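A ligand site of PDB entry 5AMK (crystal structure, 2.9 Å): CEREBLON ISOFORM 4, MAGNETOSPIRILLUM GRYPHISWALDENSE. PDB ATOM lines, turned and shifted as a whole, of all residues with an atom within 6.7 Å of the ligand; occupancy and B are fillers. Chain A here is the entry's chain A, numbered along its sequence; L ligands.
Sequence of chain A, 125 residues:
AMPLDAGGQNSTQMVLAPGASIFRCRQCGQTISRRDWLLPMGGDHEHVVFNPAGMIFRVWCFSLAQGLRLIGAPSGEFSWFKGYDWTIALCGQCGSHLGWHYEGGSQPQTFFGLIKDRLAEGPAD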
ATOM      1  N   VAL A  49      -6.843 -27.280   1.577  1.00  0.00           N
ATOM      2  CA  VAL A  49      -7.312 -25.928   1.316  1.00  0.00           C
ATOM      3  C   VAL A  49      -8.340 -25.950   0.249  1.00  0.00           C
ATOM      4  O   VAL A  49      -8.391 -26.864  -0.493  1.00  0.00           O
ATOM      5  CB  VAL A  49      -6.175 -25.045   0.818  1.00  0.00           C
ATOM      6  CG1 VAL A  49      -4.977 -25.215   1.710  1.00  0.00           C
ATOM      7  CG2 VAL A  49      -5.776 -25.455  -0.573  1.00  0.00           C
ATOM      8  N   PHE A  50      -9.145 -24.912   0.178  1.00  0.00           N
ATOM      9  CA  PHE A  50      -9.815 -24.587  -1.093  1.00  0.00           C
ATOM     10  C   PHE A  50      -9.487 -23.200  -1.587  1.00  0.00           C
ATOM     11  O   PHE A  50      -8.939 -22.422  -0.858  1.00  0.00           O
ATOM     12  CB  PHE A  50     -11.318 -24.861  -1.094  1.00  0.00           C
ATOM     13  CG  PHE A  50     -12.111 -24.180  -0.029  1.00  0.00           C
ATOM     14  CD1 PHE A  50     -12.691 -22.939  -0.256  1.00  0.00           C
ATOM     15  CD2 PHE A  50     -12.456 -24.853   1.131  1.00  0.00           C
ATOM     16  CE1 PHE A  50     -13.539 -22.333   0.696  1.00  0.00           C
ATOM     17  CE2 PHE A  50     -13.273 -24.247   2.102  1.00  0.00           C
ATOM     18  CZ  PHE A  50     -13.809 -22.981   1.881  1.00  0.00           C
ATOM     19  N   ASN A  51      -9.773 -22.959  -2.852  1.00  0.00           N
ATOM     20  CA  ASN A  51      -9.523 -21.658  -3.452  1.00  0.00           C
ATOM     21  C   ASN A  51     -10.842 -20.973  -3.848  1.00  0.00           C
ATOM     22  O   ASN A  51     -11.931 -21.523  -3.661  1.00  0.00           O
ATOM     23  CB  ASN A  51      -8.609 -21.808  -4.669  1.00  0.00           C
ATOM     24  CG  ASN A  51      -9.282 -22.588  -5.780  1.00  0.00           C
ATOM     25  OD1 ASN A  51     -10.494 -22.808  -5.733  1.00  0.00           O
ATOM     26  ND2 ASN A  51      -8.500 -23.047  -6.770  1.00  0.00           N
ATOM     27  N   PRO A  52     -10.749 -19.748  -4.403  1.00  0.00           N
ATOM     28  CA  PRO A  52     -11.939 -19.021  -4.749  1.00  0.00           C
ATOM     29  C   PRO A  52     -12.688 -19.644  -5.895  1.00  0.00           C
ATOM     30  O   PRO A  52     -13.818 -19.389  -6.047  1.00  0.00           O
ATOM     31  CB  PRO A  52     -11.387 -17.658  -5.153  1.00  0.00           C
ATOM     32  CG  PRO A  52     -10.067 -17.523  -4.468  1.00  0.00           C
ATOM     33  CD  PRO A  52      -9.552 -18.923  -4.649  1.00  0.00           C
ATOM     34  N   ALA A  53     -12.058 -20.501  -6.673  1.00  0.00           N
ATOM     35  CA  ALA A  53     -12.825 -21.295  -7.649  1.00  0.00           C
ATOM     36  C   ALA A  53     -13.651 -22.413  -7.062  1.00  0.00           C
ATOM     37  O   ALA A  53     -14.428 -23.000  -7.770  1.00  0.00           O
ATOM     38  CB  ALA A  53     -11.899 -21.890  -8.673  1.00  0.00           C
ATOM     39  N   GLY A  54     -13.462 -22.722  -5.772  1.00  0.00           N
ATOM     40  CA  GLY A  54     -14.224 -23.776  -5.105  1.00  0.00           C
ATOM     41  C   GLY A  54     -13.645 -25.162  -5.253  1.00  0.00           C
ATOM     42  O   GLY A  54     -14.302 -26.140  -4.974  1.00  0.00           O
ATOM     43  N   MET A  55     -12.385 -25.196  -5.677  1.00  0.00           N
ATOM     44  CA  MET A  55     -11.592 -26.407  -5.802  1.00  0.00           C
ATOM     45  C   MET A  55     -10.883 -26.676  -4.486  1.00  0.00           C
ATOM     46  O   MET A  55     -10.179 -25.805  -4.006  1.00  0.00           O
ATOM     47  CB  MET A  55     -10.552 -26.201  -6.931  1.00  0.00           C
ATOM     48  CG  MET A  55     -10.107 -27.463  -7.674  1.00  0.00           C
ATOM     49  SD  MET A  55     -11.365 -28.442  -8.585  1.00  0.00           S
ATOM     50  CE  MET A  55     -11.573 -29.947  -7.586  1.00  0.00           C
ATOM     51  N   PHE A  57      -7.742 -28.536  -3.163  1.00  0.00           N
ATOM     52  CA  PHE A  57      -6.428 -29.204  -3.189  1.00  0.00           C
ATOM     53  C   PHE A  57      -5.917 -29.751  -1.801  1.00  0.00           C
ATOM     54  O   PHE A  57      -6.389 -29.348  -0.753  1.00  0.00           O
ATOM     55  CB  PHE A  57      -5.331 -28.212  -3.571  1.00  0.00           C
ATOM     56  CG  PHE A  57      -5.683 -27.322  -4.657  1.00  0.00           C
ATOM     57  CD1 PHE A  57      -5.544 -27.746  -5.992  1.00  0.00           C
ATOM     58  CD2 PHE A  57      -6.087 -26.058  -4.383  1.00  0.00           C
ATOM     59  CE1 PHE A  57      -5.831 -26.904  -7.083  1.00  0.00           C
ATOM     60  CE2 PHE A  57      -6.400 -25.205  -5.428  1.00  0.00           C
ATOM     61  CZ  PHE A  57      -6.252 -25.621  -6.793  1.00  0.00           C
ATOM     62  N   SER A  75       2.189 -12.174  -5.063  1.00  0.00           N
ATOM     63  CA  SER A  75       0.831 -11.760  -4.786  1.00  0.00           C
ATOM     64  C   SER A  75       0.444 -12.297  -3.419  1.00  0.00           C
ATOM     65  O   SER A  75       0.588 -13.492  -3.155  1.00  0.00           O
ATOM     66  CB  SER A  75      -0.121 -12.380  -5.811  1.00  0.00           C
ATOM     67  OG  SER A  75       0.432 -12.459  -7.111  1.00  0.00           O
ATOM     68  N   GLU A  77      -2.770 -11.786  -2.224  1.00  0.00           N
ATOM     69  CA  GLU A  77      -4.206 -11.947  -2.174  1.00  0.00           C
ATOM     70  C   GLU A  77      -4.466 -13.431  -2.178  1.00  0.00           C
ATOM     71  O   GLU A  77      -3.767 -14.194  -2.837  1.00  0.00           O
ATOM     72  CB  GLU A  77      -4.855 -11.377  -3.395  1.00  0.00           C
ATOM     73  CG  GLU A  77      -4.031 -10.254  -4.002  1.00  0.00           C
ATOM     74  CD  GLU A  77      -3.441 -10.622  -5.334  1.00  0.00           C
ATOM     75  OE1 GLU A  77      -4.136 -11.217  -6.162  1.00  0.00           O
ATOM     76  OE2 GLU A  77      -2.295 -10.238  -5.592  1.00  0.00           O
ATOM     77  N   PHE A  78      -5.464 -13.847  -1.434  1.00  0.00           N
ATOM     78  CA  PHE A  78      -5.827 -15.239  -1.346  1.00  0.00           C
ATOM     79  C   PHE A  78      -4.779 -16.153  -0.685  1.00  0.00           C
ATOM     80  O   PHE A  78      -4.995 -17.360  -0.652  1.00  0.00           O
ATOM     81  CB  PHE A  78      -6.173 -15.810  -2.750  1.00  0.00           C
ATOM     82  CG  PHE A  78      -7.103 -14.923  -3.559  1.00  0.00           C
ATOM     83  CD1 PHE A  78      -8.361 -14.626  -3.100  1.00  0.00           C
ATOM     84  CD2 PHE A  78      -6.705 -14.397  -4.741  1.00  0.00           C
ATOM     85  CE1 PHE A  78      -9.203 -13.815  -3.829  1.00  0.00           C
ATOM     86  CE2 PHE A  78      -7.558 -13.595  -5.472  1.00  0.00           C
ATOM     87  CZ  PHE A  78      -8.796 -13.303  -5.006  1.00  0.00           C
ATOM     88  N   SER A  79      -3.669 -15.627  -0.172  1.00  0.00           N
ATOM     89  CA  SER A  79      -2.633 -16.536   0.293  1.00  0.00           C
ATOM     90  C   SER A  79      -3.163 -17.388   1.396  1.00  0.00           C
ATOM     91  O   SER A  79      -3.813 -16.865   2.287  1.00  0.00           O
ATOM     92  CB  SER A  79      -1.422 -15.769   0.832  1.00  0.00           C
ATOM     93  OG  SER A  79      -0.383 -16.676   1.183  1.00  0.00           O
ATOM     94  N   TRP A  80      -2.900 -18.702   1.362  1.00  0.00           N
ATOM     95  CA  TRP A  80      -3.294 -19.590   2.451  1.00  0.00           C
ATOM     96  C   TRP A  80      -2.402 -19.518   3.663  1.00  0.00           C
ATOM     97  O   TRP A  80      -2.782 -20.065   4.693  1.00  0.00           O
ATOM     98  CB  TRP A  80      -3.337 -21.054   2.019  1.00  0.00           C
ATOM     99  CG  TRP A  80      -4.320 -21.303   0.957  1.00  0.00           C
ATOM    100  CD1 TRP A  80      -5.662 -21.064   0.995  1.00  0.00           C
ATOM    101  CD2 TRP A  80      -4.047 -21.822  -0.327  1.00  0.00           C
ATOM    102  NE1 TRP A  80      -6.231 -21.419  -0.184  1.00  0.00           N
ATOM    103  CE2 TRP A  80      -5.259 -21.898  -1.009  1.00  0.00           C
ATOM    104  CE3 TRP A  80      -2.897 -22.268  -0.949  1.00  0.00           C
ATOM    105  CZ2 TRP A  80      -5.345 -22.381  -2.291  1.00  0.00           C
ATOM    106  CZ3 TRP A  80      -2.984 -22.747  -2.241  1.00  0.00           C
ATOM    107  CH2 TRP A  80      -4.192 -22.813  -2.889  1.00  0.00           C
ATOM    108  N   PHE A  81      -1.236 -18.862   3.545  1.00  0.00           N
ATOM    109  CA  PHE A  81      -0.255 -18.816   4.622  1.00  0.00           C
ATOM    110  C   PHE A  81       0.084 -17.397   5.042  1.00  0.00           C
ATOM    111  O   PHE A  81       0.537 -16.599   4.238  1.00  0.00           O
ATOM    112  CB  PHE A  81       1.033 -19.488   4.179  1.00  0.00           C
ATOM    113  CG  PHE A  81       0.836 -20.908   3.774  1.00  0.00           C
ATOM    114  CD1 PHE A  81       0.793 -21.908   4.726  1.00  0.00           C
ATOM    115  CD2 PHE A  81       0.672 -21.233   2.415  1.00  0.00           C
ATOM    116  CE1 PHE A  81       0.578 -23.221   4.322  1.00  0.00           C
ATOM    117  CE2 PHE A  81       0.477 -22.548   2.009  1.00  0.00           C
ATOM    118  CZ  PHE A  81       0.426 -23.537   2.964  1.00  0.00           C
ATOM    119  N   TYR A  84       3.085 -14.500   3.787  1.00  0.00           N
ATOM    120  CA  TYR A  84       3.759 -15.002   2.590  1.00  0.00           C
ATOM    121  C   TYR A  84       2.997 -14.609   1.342  1.00  0.00           C
ATOM    122  O   TYR A  84       1.786 -14.848   1.269  1.00  0.00           O
ATOM    123  CB  TYR A  84       3.840 -16.531   2.624  1.00  0.00           C
ATOM    124  CG  TYR A  84       4.783 -17.065   3.659  1.00  0.00           C
ATOM    125  CD1 TYR A  84       6.155 -17.104   3.417  1.00  0.00           C
ATOM    126  CD2 TYR A  84       4.321 -17.563   4.883  1.00  0.00           C
ATOM    127  CE1 TYR A  84       7.038 -17.584   4.365  1.00  0.00           C
ATOM    128  CE2 TYR A  84       5.192 -18.065   5.836  1.00  0.00           C
ATOM    129  CZ  TYR A  84       6.557 -18.065   5.574  1.00  0.00           C
ATOM    130  OH  TYR A  84       7.460 -18.530   6.495  1.00  0.00           O
ATOM    131  N   TRP A  86       2.657 -15.245  -2.851  1.00  0.00           N
ATOM    132  CA  TRP A  86       2.863 -16.404  -3.734  1.00  0.00           C
ATOM    133  C   TRP A  86       3.112 -15.993  -5.144  1.00  0.00           C
ATOM    134  O   TRP A  86       2.659 -14.917  -5.620  1.00  0.00           O
ATOM    135  CB  TRP A  86       1.682 -17.388  -3.743  1.00  0.00           C
ATOM    136  CG  TRP A  86       0.373 -16.790  -3.987  1.00  0.00           C
ATOM    137  CD1 TRP A  86      -0.506 -16.440  -3.046  1.00  0.00           C
ATOM    138  CD2 TRP A  86      -0.246 -16.480  -5.232  1.00  0.00           C
ATOM    139  NE1 TRP A  86      -1.622 -15.925  -3.602  1.00  0.00           N
ATOM    140  CE2 TRP A  86      -1.477 -15.924  -4.960  1.00  0.00           C
ATOM    141  CE3 TRP A  86       0.139 -16.602  -6.561  1.00  0.00           C
ATOM    142  CZ2 TRP A  86      -2.339 -15.495  -5.955  1.00  0.00           C
ATOM    143  CZ3 TRP A  86      -0.713 -16.178  -7.546  1.00  0.00           C
ATOM    144  CH2 TRP A  86      -1.935 -15.653  -7.242  1.00  0.00           C
ATOM    145  N   ILE A  88       3.225 -18.389  -8.923  1.00  0.00           N
ATOM    146  CA  ILE A  88       2.842 -19.689  -9.443  1.00  0.00           C
ATOM    147  C   ILE A  88       4.075 -20.412  -9.867  1.00  0.00           C
ATOM    148  O   ILE A  88       4.913 -19.835 -10.549  1.00  0.00           O
ATOM    149  CB  ILE A  88       2.019 -19.547 -10.740  1.00  0.00           C
ATOM    150  CG1 ILE A  88       0.618 -19.011 -10.427  1.00  0.00           C
ATOM    151  CG2 ILE A  88       1.911 -20.861 -11.523  1.00  0.00           C
ATOM    152  CD1 ILE A  88      -0.104 -18.528 -11.682  1.00  0.00           C
ATOM    153  N   HIS A  97       1.092 -26.949 -14.018  1.00  0.00           N
ATOM    154  CA  HIS A  97       0.996 -26.172 -12.801  1.00  0.00           C
ATOM    155  C   HIS A  97       1.129 -27.097 -11.604  1.00  0.00           C
ATOM    156  O   HIS A  97       0.199 -27.833 -11.278  1.00  0.00           O
ATOM    157  CB  HIS A  97      -0.330 -25.467 -12.712  1.00  0.00           C
ATOM    158  CG  HIS A  97      -0.437 -24.589 -11.518  1.00  0.00           C
ATOM    159  ND1 HIS A  97      -1.611 -24.384 -10.849  1.00  0.00           N
ATOM    160  CD2 HIS A  97       0.501 -23.897 -10.847  1.00  0.00           C
ATOM    161  CE1 HIS A  97      -1.405 -23.595  -9.815  1.00  0.00           C
ATOM    162  NE2 HIS A  97      -0.126 -23.266  -9.791  1.00  0.00           N
ATOM    163  N   TRP A 100       2.856 -23.498  -5.942  1.00  0.00           N
ATOM    164  CA  TRP A 100       3.405 -22.148  -5.745  1.00  0.00           C
ATOM    165  C   TRP A 100       4.673 -22.041  -4.869  1.00  0.00           C
ATOM    166  O   TRP A 100       4.979 -22.925  -4.040  1.00  0.00           O
ATOM    167  CB  TRP A 100       2.335 -21.260  -5.132  1.00  0.00           C
ATOM    168  CG  TRP A 100       1.005 -21.331  -5.778  1.00  0.00           C
ATOM    169  CD1 TRP A 100       0.500 -20.421  -6.603  1.00  0.00           C
ATOM    170  CD2 TRP A 100      -0.004 -22.317  -5.605  1.00  0.00           C
ATOM    171  NE1 TRP A 100      -0.743 -20.770  -6.978  1.00  0.00           N
ATOM    172  CE2 TRP A 100      -1.090 -21.943  -6.379  1.00  0.00           C
ATOM    173  CE3 TRP A 100      -0.099 -23.492  -4.858  1.00  0.00           C
ATOM    174  CZ2 TRP A 100      -2.278 -22.685  -6.463  1.00  0.00           C
ATOM    175  CZ3 TRP A 100      -1.270 -24.258  -4.939  1.00  0.00           C
ATOM    176  CH2 TRP A 100      -2.345 -23.855  -5.748  1.00  0.00           C
ATOM    177  N   TYR A 102       6.413 -19.569  -2.063  1.00  0.00           N
ATOM    178  CA  TYR A 102       6.042 -18.603  -1.053  1.00  0.00           C
ATOM    179  C   TYR A 102       7.283 -17.901  -0.556  1.00  0.00           C
ATOM    180  O   TYR A 102       8.307 -18.523  -0.319  1.00  0.00           O
ATOM    181  CB  TYR A 102       5.271 -19.287   0.085  1.00  0.00           C
ATOM    182  CG  TYR A 102       3.897 -19.782  -0.338  1.00  0.00           C
ATOM    183  CD1 TYR A 102       2.784 -18.962  -0.275  1.00  0.00           C
ATOM    184  CD2 TYR A 102       3.733 -21.047  -0.824  1.00  0.00           C
ATOM    185  CE1 TYR A 102       1.536 -19.411  -0.699  1.00  0.00           C
ATOM    186  CE2 TYR A 102       2.504 -21.511  -1.242  1.00  0.00           C
ATOM    187  CZ  TYR A 102       1.421 -20.691  -1.190  1.00  0.00           C
ATOM    188  OH  TYR A 102       0.219 -21.174  -1.626  1.00  0.00           O
ATOM    189  N   ILE A 115       0.908 -29.012  -5.038  1.00  0.00           N
ATOM    190  CA  ILE A 115      -0.367 -29.731  -5.092  1.00  0.00           C
ATOM    191  C   ILE A 115      -0.098 -31.232  -5.170  1.00  0.00           C
ATOM    192  O   ILE A 115       0.327 -31.711  -6.186  1.00  0.00           O
ATOM    193  CB  ILE A 115      -1.196 -29.240  -6.320  1.00  0.00           C
ATOM    194  CG1 ILE A 115      -1.248 -27.709  -6.375  1.00  0.00           C
ATOM    195  CG2 ILE A 115      -2.608 -29.802  -6.272  1.00  0.00           C
ATOM    196  CD1 ILE A 115      -2.035 -27.149  -7.532  1.00  0.00           C
HETATM  197  O1  LIG L   1      -6.079 -19.406  -3.418  1.00  0.00           O
HETATM  198  C1  LIG L   1      -4.868 -19.507  -3.548  1.00  0.00           C
HETATM  199  N1  LIG L   1      -4.028 -19.330  -2.387  1.00  0.00           N
HETATM  200  C2  LIG L   1      -2.594 -19.423  -2.501  1.00  0.00           C
HETATM  201  O2  LIG L   1      -1.868 -19.258  -1.538  1.00  0.00           O
HETATM  202  C3  LIG L   1      -2.009 -19.714  -3.884  1.00  0.00           C
HETATM  203  C4  LIG L   1      -2.885 -19.031  -4.919  1.00  0.00           C
HETATM  204  C5  LIG L   1      -4.163 -19.825  -4.890  1.00  0.00           C
HETATM  205  N2  LIG L   1      -5.179 -19.519  -5.864  1.00  0.00           N
HETATM  206  C6  LIG L   1      -8.653 -19.100  -8.894  1.00  0.00           C
HETATM  207  C7  LIG L   1      -7.879 -20.087  -8.287  1.00  0.00           C
HETATM  208  C8  LIG L   1      -6.927 -19.670  -7.394  1.00  0.00           C
HETATM  209  C9  LIG L   1      -6.700 -18.313  -7.186  1.00  0.00           C
HETATM  210  O3  LIG L   1      -5.884 -21.800  -6.543  1.00  0.00           O
HETATM  211  O4  LIG L   1      -5.095 -17.013  -5.683  1.00  0.00           O
HETATM  212  C10 LIG L   1      -7.488 -17.308  -7.735  1.00  0.00           C
HETATM  213  C11 LIG L   1      -8.480 -17.736  -8.609  1.00  0.00           C
HETATM  214  C12 LIG L   1      -5.710 -18.192  -6.119  1.00  0.00           C
HETATM  215  C13 LIG L   1      -5.911 -20.444  -6.692  1.00  0.00           C
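O of Phe 78 is in hydrogen-bond range of N1 of the ligand.
The side-chain hydroxyl (OH) of Tyr 102 is in hydrogen-bond range of an oxygen (O2) of the ligand, 2.8 Å away.
The side-chain amide nitrogen (ND2) of Asn 51 sits at hydrogen-bond distance from an oxygen (O3) of the ligand, 2.9 Å away.
An oxygen (O2) of the ligand lies within hydrogen-bond range of the backbone NH (N) of Trp 80, 3.1 Å away.
N of Ala 53 sits at hydrogen-bond distance from OD1 of Asn 51 (2.9 Å).
The backbone NH (N) of Met 55 is in hydrogen-bond range of the side-chain amide oxygen (OD1) of Asn 51 (3.0 Å).
The side-chain amide oxygen (OD1) of Asn 51 is in hydrogen-bond range of the backbone NH (N) of Gly 54 (3.0 Å).
The indole nitrogen (NE1) of Trp 86 is in hydrogen-bond range of the backbone carbonyl oxygen (O) of Glu 77 (2.9 Å).
The backbone NH of Trp 86 sits at hydrogen-bond distance from the backbone carbonyl oxygen of Ser 75.
The side-chain hydroxyl (OG) of Ser 79 is in hydrogen-bond range of the backbone carbonyl oxygen (O) of Phe 81 (3.2 Å).
OG of Ser 79 is in hydrogen-bond range of O of Tyr 84 (2.8 Å).
The backbone NH (N) of Val 49 sits at hydrogen-bond distance from the backbone carbonyl oxygen (O) of Phe 57, at 3.1 Å.
Pro 52 touches the ligand (CD to O1, 3.7 Å).
CE2 of Phe 57 touches O3 of the ligand, 3.6 Å away.
Ser 79 touches the ligand.
Trp 86 touches the ligand (CZ2 to O4, 3.2 Å).
Trp 100 touches the ligand (NE1 to C4, 3.4 Å).
Hydrophobic or aromatic side chains within 4 Å of the ligand: Pro 52, Phe 57, Phe 78, Trp 80, Trp 86, Trp 100 and Tyr 102.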
